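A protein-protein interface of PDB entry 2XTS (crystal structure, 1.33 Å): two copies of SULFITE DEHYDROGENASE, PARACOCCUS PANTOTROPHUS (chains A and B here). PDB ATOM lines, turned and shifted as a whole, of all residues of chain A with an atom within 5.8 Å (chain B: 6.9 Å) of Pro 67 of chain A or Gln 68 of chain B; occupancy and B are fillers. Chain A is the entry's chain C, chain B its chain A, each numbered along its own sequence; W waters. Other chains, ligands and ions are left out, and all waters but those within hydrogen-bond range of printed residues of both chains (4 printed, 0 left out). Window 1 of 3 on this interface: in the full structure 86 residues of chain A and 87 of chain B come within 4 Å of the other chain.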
ATOM      1  N   TYR A  27      -9.703  10.082 -21.203  1.00  0.00           N
ATOM      2  CA  TYR A  27      -8.691   9.044 -21.376  1.00  0.00           C
ATOM      3  C   TYR A  27      -8.690   8.641 -22.841  1.00  0.00           C
ATOM      4  O   TYR A  27      -9.630   8.026 -23.332  1.00  0.00           O
ATOM      5  CB  TYR A  27      -8.937   7.818 -20.480  1.00  0.00           C
ATOM      6  CG  TYR A  27      -7.664   7.026 -20.295  1.00  0.00           C
ATOM      7  CD1 TYR A  27      -7.184   6.191 -21.294  1.00  0.00           C
ATOM      8  CD2 TYR A  27      -6.938   7.093 -19.119  1.00  0.00           C
ATOM      9  CE1 TYR A  27      -6.023   5.507 -21.163  1.00  0.00           C
ATOM     10  CE2 TYR A  27      -5.751   6.409 -18.974  1.00  0.00           C
ATOM     11  CZ  TYR A  27      -5.305   5.596 -19.989  1.00  0.00           C
ATOM     12  OH  TYR A  27      -4.124   4.888 -19.881  1.00  0.00           O
ATOM     13  N   GLY A  28      -7.657   9.044 -23.566  1.00  0.00           N
ATOM     14  CA  GLY A  28      -7.639   8.934 -25.024  1.00  0.00           C
ATOM     15  C   GLY A  28      -7.123   7.628 -25.577  1.00  0.00           C
ATOM     16  O   GLY A  28      -6.450   6.869 -24.909  1.00  0.00           O
ATOM     17  N   LEU A  61       5.800  -0.470 -33.984  1.00  0.00           N
ATOM     18  CA  LEU A  61       6.286   0.268 -32.829  1.00  0.00           C
ATOM     19  C   LEU A  61       7.725   0.729 -33.059  1.00  0.00           C
ATOM     20  O   LEU A  61       8.454   0.195 -33.886  1.00  0.00           O
ATOM     21  CB  LEU A  61       6.156  -0.589 -31.559  1.00  0.00           C
ATOM     22  CG  LEU A  61       4.742  -1.057 -31.210  1.00  0.00           C
ATOM     23  CD1 LEU A  61       4.793  -1.993 -30.022  1.00  0.00           C
ATOM     24  CD2 LEU A  61       3.773   0.093 -30.962  1.00  0.00           C
ATOM     25  N   ILE A  65       9.418   1.053 -25.149  1.00  0.00           N
ATOM     26  CA  ILE A  65       8.257   0.940 -24.269  1.00  0.00           C
ATOM     27  C   ILE A  65       7.077   0.442 -25.087  1.00  0.00           C
ATOM     28  O   ILE A  65       6.743   1.023 -26.108  1.00  0.00           O
ATOM     29  CB  ILE A  65       7.913   2.311 -23.637  1.00  0.00           C
ATOM     30  CG1 ILE A  65       9.044   2.791 -22.715  1.00  0.00           C
ATOM     31  CG2 ILE A  65       6.556   2.278 -22.943  1.00  0.00           C
ATOM     32  CD1 ILE A  65       9.311   1.910 -21.516  1.00  0.00           C
ATOM     33  N   THR A  66       6.432  -0.637 -24.663  1.00  0.00           N
ATOM     34  CA  THR A  66       5.256  -1.139 -25.364  1.00  0.00           C
ATOM     35  C   THR A  66       4.007  -0.426 -24.835  1.00  0.00           C
ATOM     36  O   THR A  66       3.795  -0.428 -23.619  1.00  0.00           O
ATOM     37  CB  THR A  66       5.037  -2.649 -25.119  1.00  0.00           C
ATOM     38  OG1 THR A  66       6.265  -3.361 -25.259  1.00  0.00           O
ATOM     39  CG2 THR A  66       4.013  -3.196 -26.107  1.00  0.00           C
ATOM     40  N   PRO A  67       3.203   0.201 -25.714  1.00  0.00           N
ATOM     41  CA  PRO A  67       1.933   0.746 -25.232  1.00  0.00           C
ATOM     42  C   PRO A  67       1.067  -0.364 -24.650  1.00  0.00           C
ATOM     43  O   PRO A  67       0.802  -1.361 -25.325  1.00  0.00           O
ATOM     44  CB  PRO A  67       1.294   1.364 -26.477  1.00  0.00           C
ATOM     45  CG  PRO A  67       2.368   1.475 -27.478  1.00  0.00           C
ATOM     46  CD  PRO A  67       3.323   0.332 -27.169  1.00  0.00           C
ATOM     47  N   GLN A  68       0.618  -0.215 -23.418  1.00  0.00           N
ATOM     48  CA  GLN A  68      -0.014  -1.301 -22.730  1.00  0.00           C
ATOM     49  C   GLN A  68      -1.329  -1.709 -23.397  1.00  0.00           C
ATOM     50  O   GLN A  68      -1.708  -2.877 -23.320  1.00  0.00           O
ATOM     51  CB  GLN A  68      -0.155  -0.988 -21.237  1.00  0.00           C
ATOM     52  CG  GLN A  68      -0.701   0.359 -20.889  1.00  0.00           C
ATOM     53  CD  GLN A  68       0.372   1.417 -20.661  1.00  0.00           C
ATOM     54  OE1 GLN A  68       1.403   1.432 -21.318  1.00  0.00           O
ATOM     55  NE2 GLN A  68       0.120   2.306 -19.731  1.00  0.00           N
ATOM     56  N   GLY A  69      -1.994  -0.782 -24.082  1.00  0.00           N
ATOM     57  CA  GLY A  69      -3.216  -1.134 -24.818  1.00  0.00           C
ATOM     58  C   GLY A  69      -3.041  -2.117 -25.948  1.00  0.00           C
ATOM     59  O   GLY A  69      -4.000  -2.787 -26.308  1.00  0.00           O
ATOM     60  N   CYS A  70      -1.837  -2.211 -26.501  1.00  0.00           N
ATOM     61  CA  CYS A  70      -1.566  -3.188 -27.579  1.00  0.00           C
ATOM     62  C   CYS A  70      -0.512  -4.212 -27.181  1.00  0.00           C
ATOM     63  O   CYS A  70      -0.063  -4.964 -28.028  1.00  0.00           O
ATOM     64  CB  CYS A  70      -1.233  -2.523 -28.914  1.00  0.00           C
ATOM     65  SG  CYS A  70       0.238  -1.553 -28.934  1.00  0.00           S
ATOM     66  N   ALA A  71      -0.156  -4.249 -25.905  1.00  0.00           N
ATOM     67  CA  ALA A  71       0.772  -5.249 -25.378  1.00  0.00           C
ATOM     68  C   ALA A  71       0.072  -6.617 -25.301  1.00  0.00           C
ATOM     69  O   ALA A  71      -1.051  -6.710 -24.814  1.00  0.00           O
ATOM     70  CB  ALA A  71       1.285  -4.823 -24.035  1.00  0.00           C
ATOM     71  N   MET A 146       7.737  -3.089 -20.295  1.00  0.00           N
ATOM     72  CA  MET A 146       7.130  -2.029 -19.510  1.00  0.00           C
ATOM     73  C   MET A 146       8.008  -1.643 -18.323  1.00  0.00           C
ATOM     74  O   MET A 146       8.831  -2.418 -17.840  1.00  0.00           O
ATOM     75  CB  MET A 146       5.752  -2.442 -18.991  1.00  0.00           C
ATOM     76  CG  MET A 146       4.844  -2.975 -20.084  1.00  0.00           C
ATOM     77  SD  MET A 146       3.142  -3.218 -19.516  1.00  0.00           S
ATOM     78  CE  MET A 146       2.425  -3.980 -20.976  1.00  0.00           C
ATOM     79  N   ASN A 199       4.027   1.009 -16.813  1.00  0.00           N
ATOM     80  CA  ASN A 199       4.034   2.203 -17.643  1.00  0.00           C
ATOM     81  C   ASN A 199       3.170   3.297 -17.018  1.00  0.00           C
ATOM     82  O   ASN A 199       2.310   3.908 -17.681  1.00  0.00           O
ATOM     83  CB  ASN A 199       3.603   1.902 -19.072  1.00  0.00           C
ATOM     84  CG  ASN A 199       4.639   1.097 -19.835  1.00  0.00           C
ATOM     85  OD1 ASN A 199       5.822   1.019 -19.454  1.00  0.00           O
ATOM     86  ND2 ASN A 199       4.197   0.530 -20.970  1.00  0.00           N
ATOM     87  N   TYR B  27      -7.276  -3.145 -29.006  1.00  0.00           N
ATOM     88  CA  TYR B  27      -6.541  -2.039 -28.417  1.00  0.00           C
ATOM     89  C   TYR B  27      -7.299  -1.655 -27.136  1.00  0.00           C
ATOM     90  O   TYR B  27      -8.409  -1.101 -27.183  1.00  0.00           O
ATOM     91  CB  TYR B  27      -6.400  -0.844 -29.365  1.00  0.00           C
ATOM     92  CG  TYR B  27      -5.257   0.051 -28.931  1.00  0.00           C
ATOM     93  CD1 TYR B  27      -5.365   0.858 -27.800  1.00  0.00           C
ATOM     94  CD2 TYR B  27      -4.038   0.035 -29.593  1.00  0.00           C
ATOM     95  CE1 TYR B  27      -4.322   1.644 -27.369  1.00  0.00           C
ATOM     96  CE2 TYR B  27      -2.979   0.812 -29.178  1.00  0.00           C
ATOM     97  CZ  TYR B  27      -3.120   1.623 -28.055  1.00  0.00           C
ATOM     98  OH  TYR B  27      -2.105   2.399 -27.580  1.00  0.00           O
ATOM     99  N   ARG B  39      -7.545  12.581 -17.457  1.00  0.00           N
ATOM    100  CA  ARG B  39      -7.327  14.009 -17.533  1.00  0.00           C
ATOM    101  C   ARG B  39      -8.507  14.728 -16.925  1.00  0.00           C
ATOM    102  O   ARG B  39      -9.651  14.322 -17.118  1.00  0.00           O
ATOM    103  CB  ARG B  39      -7.209  14.480 -18.964  1.00  0.00           C
ATOM    104  CG  ARG B  39      -6.113  13.856 -19.731  1.00  0.00           C
ATOM    105  CD  ARG B  39      -6.603  13.657 -21.192  1.00  0.00           C
ATOM    106  NE  ARG B  39      -5.488  13.403 -22.021  1.00  0.00           N
ATOM    107  CZ  ARG B  39      -5.518  12.936 -23.256  1.00  0.00           C
ATOM    108  NH1 ARG B  39      -4.360  12.837 -23.837  1.00  0.00           N
ATOM    109  NH2 ARG B  39      -6.643  12.567 -23.885  1.00  0.00           N
ATOM    110  N   ILE B  65       7.073   6.956 -16.591  1.00  0.00           N
ATOM    111  CA  ILE B  65       6.457   7.024 -17.913  1.00  0.00           C
ATOM    112  C   ILE B  65       5.004   7.435 -17.774  1.00  0.00           C
ATOM    113  O   ILE B  65       4.258   6.810 -17.021  1.00  0.00           O
ATOM    114  CB  ILE B  65       6.531   5.639 -18.612  1.00  0.00           C
ATOM    115  CG1 ILE B  65       7.990   5.258 -18.907  1.00  0.00           C
ATOM    116  CG2 ILE B  65       5.689   5.611 -19.882  1.00  0.00           C
ATOM    117  CD1 ILE B  65       8.696   6.164 -19.863  1.00  0.00           C
ATOM    118  N   THR B  66       4.580   8.492 -18.473  1.00  0.00           N
ATOM    119  CA  THR B  66       3.181   8.890 -18.411  1.00  0.00           C
ATOM    120  C   THR B  66       2.385   8.112 -19.454  1.00  0.00           C
ATOM    121  O   THR B  66       2.751   8.133 -20.625  1.00  0.00           O
ATOM    122  CB  THR B  66       3.003  10.398 -18.741  1.00  0.00           C
ATOM    123  OG1 THR B  66       3.957  11.196 -18.016  1.00  0.00           O
ATOM    124  CG2 THR B  66       1.561  10.840 -18.391  1.00  0.00           C
ATOM    125  N   PRO B  67       1.271   7.457 -19.051  1.00  0.00           N
ATOM    126  CA  PRO B  67       0.431   6.823 -20.089  1.00  0.00           C
ATOM    127  C   PRO B  67      -0.111   7.879 -21.023  1.00  0.00           C
ATOM    128  O   PRO B  67      -0.693   8.844 -20.582  1.00  0.00           O
ATOM    129  CB  PRO B  67      -0.685   6.150 -19.279  1.00  0.00           C
ATOM    130  CG  PRO B  67      -0.179   6.098 -17.897  1.00  0.00           C
ATOM    131  CD  PRO B  67       0.674   7.294 -17.708  1.00  0.00           C
ATOM    132  N   GLN B  68       0.082   7.707 -22.313  1.00  0.00           N
ATOM    133  CA  GLN B  68      -0.222   8.756 -23.238  1.00  0.00           C
ATOM    134  C   GLN B  68      -1.703   9.082 -23.292  1.00  0.00           C
ATOM    135  O   GLN B  68      -2.058  10.225 -23.579  1.00  0.00           O
ATOM    136  CB  GLN B  68       0.378   8.492 -24.626  1.00  0.00           C
ATOM    137  CG  GLN B  68       0.189   7.107 -25.175  1.00  0.00           C
ATOM    138  CD  GLN B  68       1.299   6.119 -24.842  1.00  0.00           C
ATOM    139  OE1 GLN B  68       1.893   6.166 -23.763  1.00  0.00           O
ATOM    140  NE2 GLN B  68       1.591   5.238 -25.781  1.00  0.00           N
ATOM    141  N   GLY B  69      -2.564   8.123 -22.988  1.00  0.00           N
ATOM    142  CA  GLY B  69      -3.975   8.407 -22.966  1.00  0.00           C
ATOM    143  C   GLY B  69      -4.428   9.363 -21.875  1.00  0.00           C
ATOM    144  O   GLY B  69      -5.499   9.955 -21.996  1.00  0.00           O
ATOM    145  N   CYS B  70      -3.656   9.490 -20.798  1.00  0.00           N
ATOM    146  CA  CYS B  70      -3.990  10.492 -19.784  1.00  0.00           C
ATOM    147  C   CYS B  70      -2.950  11.579 -19.609  1.00  0.00           C
ATOM    148  O   CYS B  70      -3.001  12.344 -18.660  1.00  0.00           O
ATOM    149  CB  CYS B  70      -4.288   9.863 -18.437  1.00  0.00           C
ATOM    150  SG  CYS B  70      -2.977   8.934 -17.658  1.00  0.00           S
ATOM    151  N   ALA B  71      -2.035  11.680 -20.558  1.00  0.00           N
ATOM    152  CA  ALA B  71      -1.029  12.727 -20.583  1.00  0.00           C
ATOM    153  C   ALA B  71      -1.684  14.041 -21.007  1.00  0.00           C
ATOM    154  O   ALA B  71      -2.446  14.087 -21.986  1.00  0.00           O
ATOM    155  CB  ALA B  71       0.092  12.352 -21.520  1.00  0.00           C
ATOM    156  N   PHE B  72      -1.391  15.110 -20.266  1.00  0.00           N
ATOM    157  CA  PHE B  72      -2.085  16.382 -20.461  1.00  0.00           C
ATOM    158  C   PHE B  72      -1.988  16.901 -21.879  1.00  0.00           C
ATOM    159  O   PHE B  72      -1.062  16.561 -22.634  1.00  0.00           O
ATOM    160  CB  PHE B  72      -1.606  17.475 -19.487  1.00  0.00           C
ATOM    161  CG  PHE B  72      -0.391  18.250 -19.943  1.00  0.00           C
ATOM    162  CD1 PHE B  72       0.860  17.692 -20.010  1.00  0.00           C
ATOM    163  CD2 PHE B  72      -0.520  19.582 -20.286  1.00  0.00           C
ATOM    164  CE1 PHE B  72       1.945  18.431 -20.425  1.00  0.00           C
ATOM    165  CE2 PHE B  72       0.559  20.310 -20.689  1.00  0.00           C
ATOM    166  CZ  PHE B  72       1.789  19.758 -20.763  1.00  0.00           C
ATOM    167  N   HIS B 144       4.035  15.857 -18.744  1.00  0.00           N
ATOM    168  CA  HIS B 144       4.076  14.452 -19.114  1.00  0.00           C
ATOM    169  C   HIS B 144       5.511  14.072 -19.458  1.00  0.00           C
ATOM    170  O   HIS B 144       6.363  14.939 -19.629  1.00  0.00           O
ATOM    171  CB  HIS B 144       3.044  14.064 -20.210  1.00  0.00           C
ATOM    172  CG  HIS B 144       3.154  14.757 -21.525  1.00  0.00           C
ATOM    173  ND1 HIS B 144       4.284  14.714 -22.313  1.00  0.00           N
ATOM    174  CD2 HIS B 144       2.203  15.386 -22.250  1.00  0.00           C
ATOM    175  CE1 HIS B 144       4.029  15.337 -23.452  1.00  0.00           C
ATOM    176  NE2 HIS B 144       2.776  15.755 -23.439  1.00  0.00           N
ATOM    177  N   MET B 146       7.628  11.072 -21.708  1.00  0.00           N
ATOM    178  CA  MET B 146       7.528   9.999 -22.681  1.00  0.00           C
ATOM    179  C   MET B 146       8.893   9.690 -23.294  1.00  0.00           C
ATOM    180  O   MET B 146       9.812  10.517 -23.327  1.00  0.00           O
ATOM    181  CB  MET B 146       6.543  10.357 -23.807  1.00  0.00           C
ATOM    182  CG  MET B 146       5.215  10.816 -23.271  1.00  0.00           C
ATOM    183  SD  MET B 146       3.987  10.926 -24.585  1.00  0.00           S
ATOM    184  CE  MET B 146       2.611  11.605 -23.660  1.00  0.00           C
ATOM    185  N   ALA B 198       5.990   8.242 -29.542  1.00  0.00           N
ATOM    186  CA  ALA B 198       6.011   8.569 -28.115  1.00  0.00           C
ATOM    187  C   ALA B 198       5.489   7.354 -27.376  1.00  0.00           C
ATOM    188  O   ALA B 198       4.384   6.874 -27.635  1.00  0.00           O
ATOM    189  CB  ALA B 198       5.172   9.787 -27.827  1.00  0.00           C
ATOM    190  N   ASN B 199       6.297   6.825 -26.469  1.00  0.00           N
ATOM    191  CA  ASN B 199       6.004   5.623 -25.692  1.00  0.00           C
ATOM    192  C   ASN B 199       5.618   4.476 -26.639  1.00  0.00           C
ATOM    193  O   ASN B 199       4.591   3.812 -26.460  1.00  0.00           O
ATOM    194  CB  ASN B 199       4.924   5.907 -24.653  1.00  0.00           C
ATOM    195  CG  ASN B 199       5.427   6.727 -23.497  1.00  0.00           C
ATOM    196  OD1 ASN B 199       6.632   6.886 -23.286  1.00  0.00           O
ATOM    197  ND2 ASN B 199       4.496   7.265 -22.728  1.00  0.00           N
ATOM    198  N   GLY B 200       6.444   4.297 -27.673  1.00  0.00           N
ATOM    199  CA  GLY B 200       6.364   3.163 -28.543  1.00  0.00           C
ATOM    200  C   GLY B 200       5.602   3.317 -29.834  1.00  0.00           C
ATOM    201  O   GLY B 200       5.899   2.654 -30.802  1.00  0.00           O
ATOM    202  N   GLU B 201       4.564   4.129 -29.840  1.00  0.00           N
ATOM    203  CA  GLU B 201       3.625   4.223 -30.949  1.00  0.00           C
ATOM    204  C   GLU B 201       3.573   5.654 -31.486  1.00  0.00           C
ATOM    205  O   GLU B 201       4.229   6.554 -30.969  1.00  0.00           O
ATOM    206  CB  GLU B 201       2.246   3.745 -30.482  1.00  0.00           C
ATOM    207  CG  GLU B 201       1.648   4.576 -29.356  1.00  0.00           C
ATOM    208  CD  GLU B 201       0.312   4.082 -28.829  1.00  0.00           C
ATOM    209  OE1 GLU B 201      -0.212   3.039 -29.317  1.00  0.00           O
ATOM    210  OE2 GLU B 201      -0.183   4.760 -27.920  1.00  0.00           O
ATOM    211  N   ALA B 202       2.788   5.880 -32.522  1.00  0.00           N
ATOM    212  CA  ALA B 202       2.653   7.230 -33.043  1.00  0.00           C
ATOM    213  C   ALA B 202       2.165   8.179 -31.971  1.00  0.00           C
ATOM    214  O   ALA B 202       1.420   7.784 -31.068  1.00  0.00           O
ATOM    215  CB  ALA B 202       1.724   7.270 -34.242  1.00  0.00           C
ATOM    216  N   ARG B 204      -0.169  10.679 -30.162  1.00  0.00           N
ATOM    217  CA  ARG B 204      -1.623  10.833 -30.148  1.00  0.00           C
ATOM    218  C   ARG B 204      -2.009  12.108 -30.908  1.00  0.00           C
ATOM    219  O   ARG B 204      -1.212  13.041 -31.076  1.00  0.00           O
ATOM    220  CB  ARG B 204      -2.126  10.831 -28.697  1.00  0.00           C
ATOM    221  CG  ARG B 204      -1.796   9.572 -27.930  1.00  0.00           C
ATOM    222  CD  ARG B 204      -2.340   8.329 -28.614  1.00  0.00           C
ATOM    223  NE  ARG B 204      -2.069   7.048 -27.961  1.00  0.00           N
ATOM    224  CZ  ARG B 204      -2.828   6.528 -26.994  1.00  0.00           C
ATOM    225  NH1 ARG B 204      -3.814   7.228 -26.448  1.00  0.00           N
ATOM    226  NH2 ARG B 204      -2.556   5.320 -26.525  1.00  0.00           N
ATOM    227  N   GLU B 206      -3.842  14.558 -30.106  1.00  0.00           N
ATOM    228  CA  GLU B 206      -3.779  15.718 -29.254  1.00  0.00           C
ATOM    229  C   GLU B 206      -2.375  16.112 -28.844  1.00  0.00           C
ATOM    230  O   GLU B 206      -2.174  17.206 -28.321  1.00  0.00           O
ATOM    231  CB  GLU B 206      -4.662  15.489 -28.011  1.00  0.00           C
ATOM    232  CG  GLU B 206      -4.256  14.365 -27.065  1.00  0.00           C
ATOM    233  CD  GLU B 206      -4.802  12.993 -27.412  1.00  0.00           C
ATOM    234  OE1 GLU B 206      -5.137  12.694 -28.581  1.00  0.00           O
ATOM    235  OE2 GLU B 206      -4.885  12.188 -26.460  1.00  0.00           O
ATOM    236  N   HIS B 207      -1.418  15.221 -29.098  1.00  0.00           N
ATOM    237  CA  HIS B 207       0.000  15.455 -28.815  1.00  0.00           C
ATOM    238  C   HIS B 207       0.815  15.745 -30.074  1.00  0.00           C
ATOM    239  O   HIS B 207       2.032  15.752 -30.045  1.00  0.00           O
ATOM    240  CB  HIS B 207       0.604  14.282 -28.041  1.00  0.00           C
ATOM    241  CG  HIS B 207      -0.077  13.999 -26.738  1.00  0.00           C
ATOM    242  ND1 HIS B 207      -0.272  12.717 -26.260  1.00  0.00           N
ATOM    243  CD2 HIS B 207      -0.582  14.842 -25.807  1.00  0.00           C
ATOM    244  CE1 HIS B 207      -0.903  12.793 -25.094  1.00  0.00           C
ATOM    245  NE2 HIS B 207      -1.080  14.069 -24.790  1.00  0.00           N
HETATM  246  O   HOH W   1      -1.984   1.988 -24.809  1.00  0.00           O
HETATM  247  O   HOH W   2      -2.748   5.369 -22.294  1.00  0.00           O
HETATM  248  O   HOH W   3      -4.559   4.931 -24.344  1.00  0.00           O
HETATM  249  O   HOH W   4       1.787   4.078 -22.045  1.00  0.00           O
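Tyr 27 of chain A touches Pro 67 of chain B, and with the chains exchanged Pro 67 of chain A touches Tyr 27 of chain B. Tyr 27 of chain A touches Gly 69 of chain B, and with the chains exchanged Gly 69 of chain A touches Tyr 27 of chain B. Tyr 27 of chain A touches Cys 70 of chain B, and with the chains exchanged Cys 70 of chain A touches Tyr 27 of chain B. Pro 67 of chain A touches Asn 199 of chain B, and with the chains exchanged Asn 199 of chain A touches Pro 67 of chain B. Of the 19 pairs that touch across the chains among the printed residues, 12 have their exchanged pair printed and touching as well.
The guanidinium group (NH2) of Arg 204 of chain B lies within hydrogen-bond range of the side-chain hydroxyl (OH) of Tyr 27 of chain B (3.1 Å). The guanidinium group (NH1) of Arg 39 of chain B lies within salt-bridge range of the side-chain carboxylate (OE2) of Glu 206 of chain B (2.8 Å). The backbone carbonyl oxygen of Gln 68 of chain B is in hydrogen-bond range of the guanidinium group of Arg 39 of chain B, at 3.5 Å. The side-chain carboxylate (OE2) of Glu 201 of chain B lies within salt-bridge range of the guanidinium group (NH2) of Arg 204 of chain B, 2.8 Å away. The backbone carbonyl oxygen (O) of Thr 66 of chain B is in hydrogen-bond range of the side-chain amide nitrogen (ND2) of Asn 199 of chain B (2.9 Å). The side-chain amide nitrogen of Asn 199 of chain A sits at hydrogen-bond distance from the backbone carbonyl oxygen of Thr 66 of chain A (2.8 Å).
Hydrophobic or aromatic side chains of chain B within 4 Å of the printed part of chain A: Tyr 27 and Pro 67. Printed residues of chain A that touch a printed residue of chain B: Tyr 27, Gly 28, Leu 61, Ile 65, Pro 67, Gln 68, Gly 69, Cys 70 and Asn 199. Among the printed residues, no Asp or Glu carboxylate lies within 4 Å of a Lys or Arg side-chain nitrogen of the other chain.
Water W4 bridges the side-chain amide oxygen of Gln 68 of chain B (2.7 Å) and the side-chain amide oxygen of Gln 68 of chain A (2.8 Å). Water W3 lies within hydrogen-bond range of the backbone carbonyl oxygen of Gly 28 of chain A (2.8 Å) and the guanidinium group of Arg 204 of chain B (3.0 Å). Water W1 lies within hydrogen-bond range of OH of Tyr 27 of chain B (2.8 Å) and N of Gly 69 of chain A (2.9 Å). Water W2 bridges OH of Tyr 27 of chain A and N of Gly 69 of chain B.
Printed residues of chain A within 4 Å of Arg 204 of chain B: Gly 28 (3.1 Å). Printed residues of chain A within 4 Å of Cys 70 of chain B: Tyr 27. Printed residues of chain A within 4 Å of Pro 67 of chain B: Tyr 27 (3.7 Å), Gln 68 (3.95 Å) and Asn 199 (3.3 Å). Of the printed residues of chain B, Leu 61 of chain A touches Gly 200 and Glu 201. The nearest residue of chain A that does not touch Gln 68 of chain B is Gln 68 of chain A (5.4 Å).
Among the printed residues, pairs that only touch across the chains: Tyr 27 of chain A with Pro 67 of chain B (3.7 Å), Tyr 27 of chain A with Gly 69 of chain B (3.4 Å), Tyr 27 of chain A with Cys 70 of chain B (3.8 Å), Gly 28 of chain A with Arg 39 of chain B (3.7 Å), Leu 61 of chain A with Gly 200 of chain B (3.2 Å), Leu 61 of chain A with Glu 201 of chain B (3.99 Å), Ile 65 of chain A with Asn 199 of chain B (3.5 Å), Ile 65 of chain A with Gly 200 of chain B (3.3 Å), Pro 67 of chain A with Tyr 27 of chain B (3.7 Å), Pro 67 of chain A with Gln 68 of chain B (3.9 Å), Pro 67 of chain A with Asn 199 of chain B (3.4 Å), Pro 67 of chain A with Glu 201 of chain B (3.5 Å), Gln 68 of chain A with Pro 67 of chain B (3.95 Å), Gly 69 of chain A with Tyr 27 of chain B (3.4 Å), Cys 70 of chain A with Tyr 27 of chain B (3.8 Å), Asn 199 of chain A with Ile 65 of chain B (3.6 Å) and Asn 199 of chain A with Pro 67 of chain B (3.3 Å).
N of Gly 28 of chain A is in hydrogen-bond range of O of Gly 69 of chain B (2.8 Å). NH1 of Arg 204 of chain B is in hydrogen-bond range of O of Gly 28 of chain A (3.1 Å).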
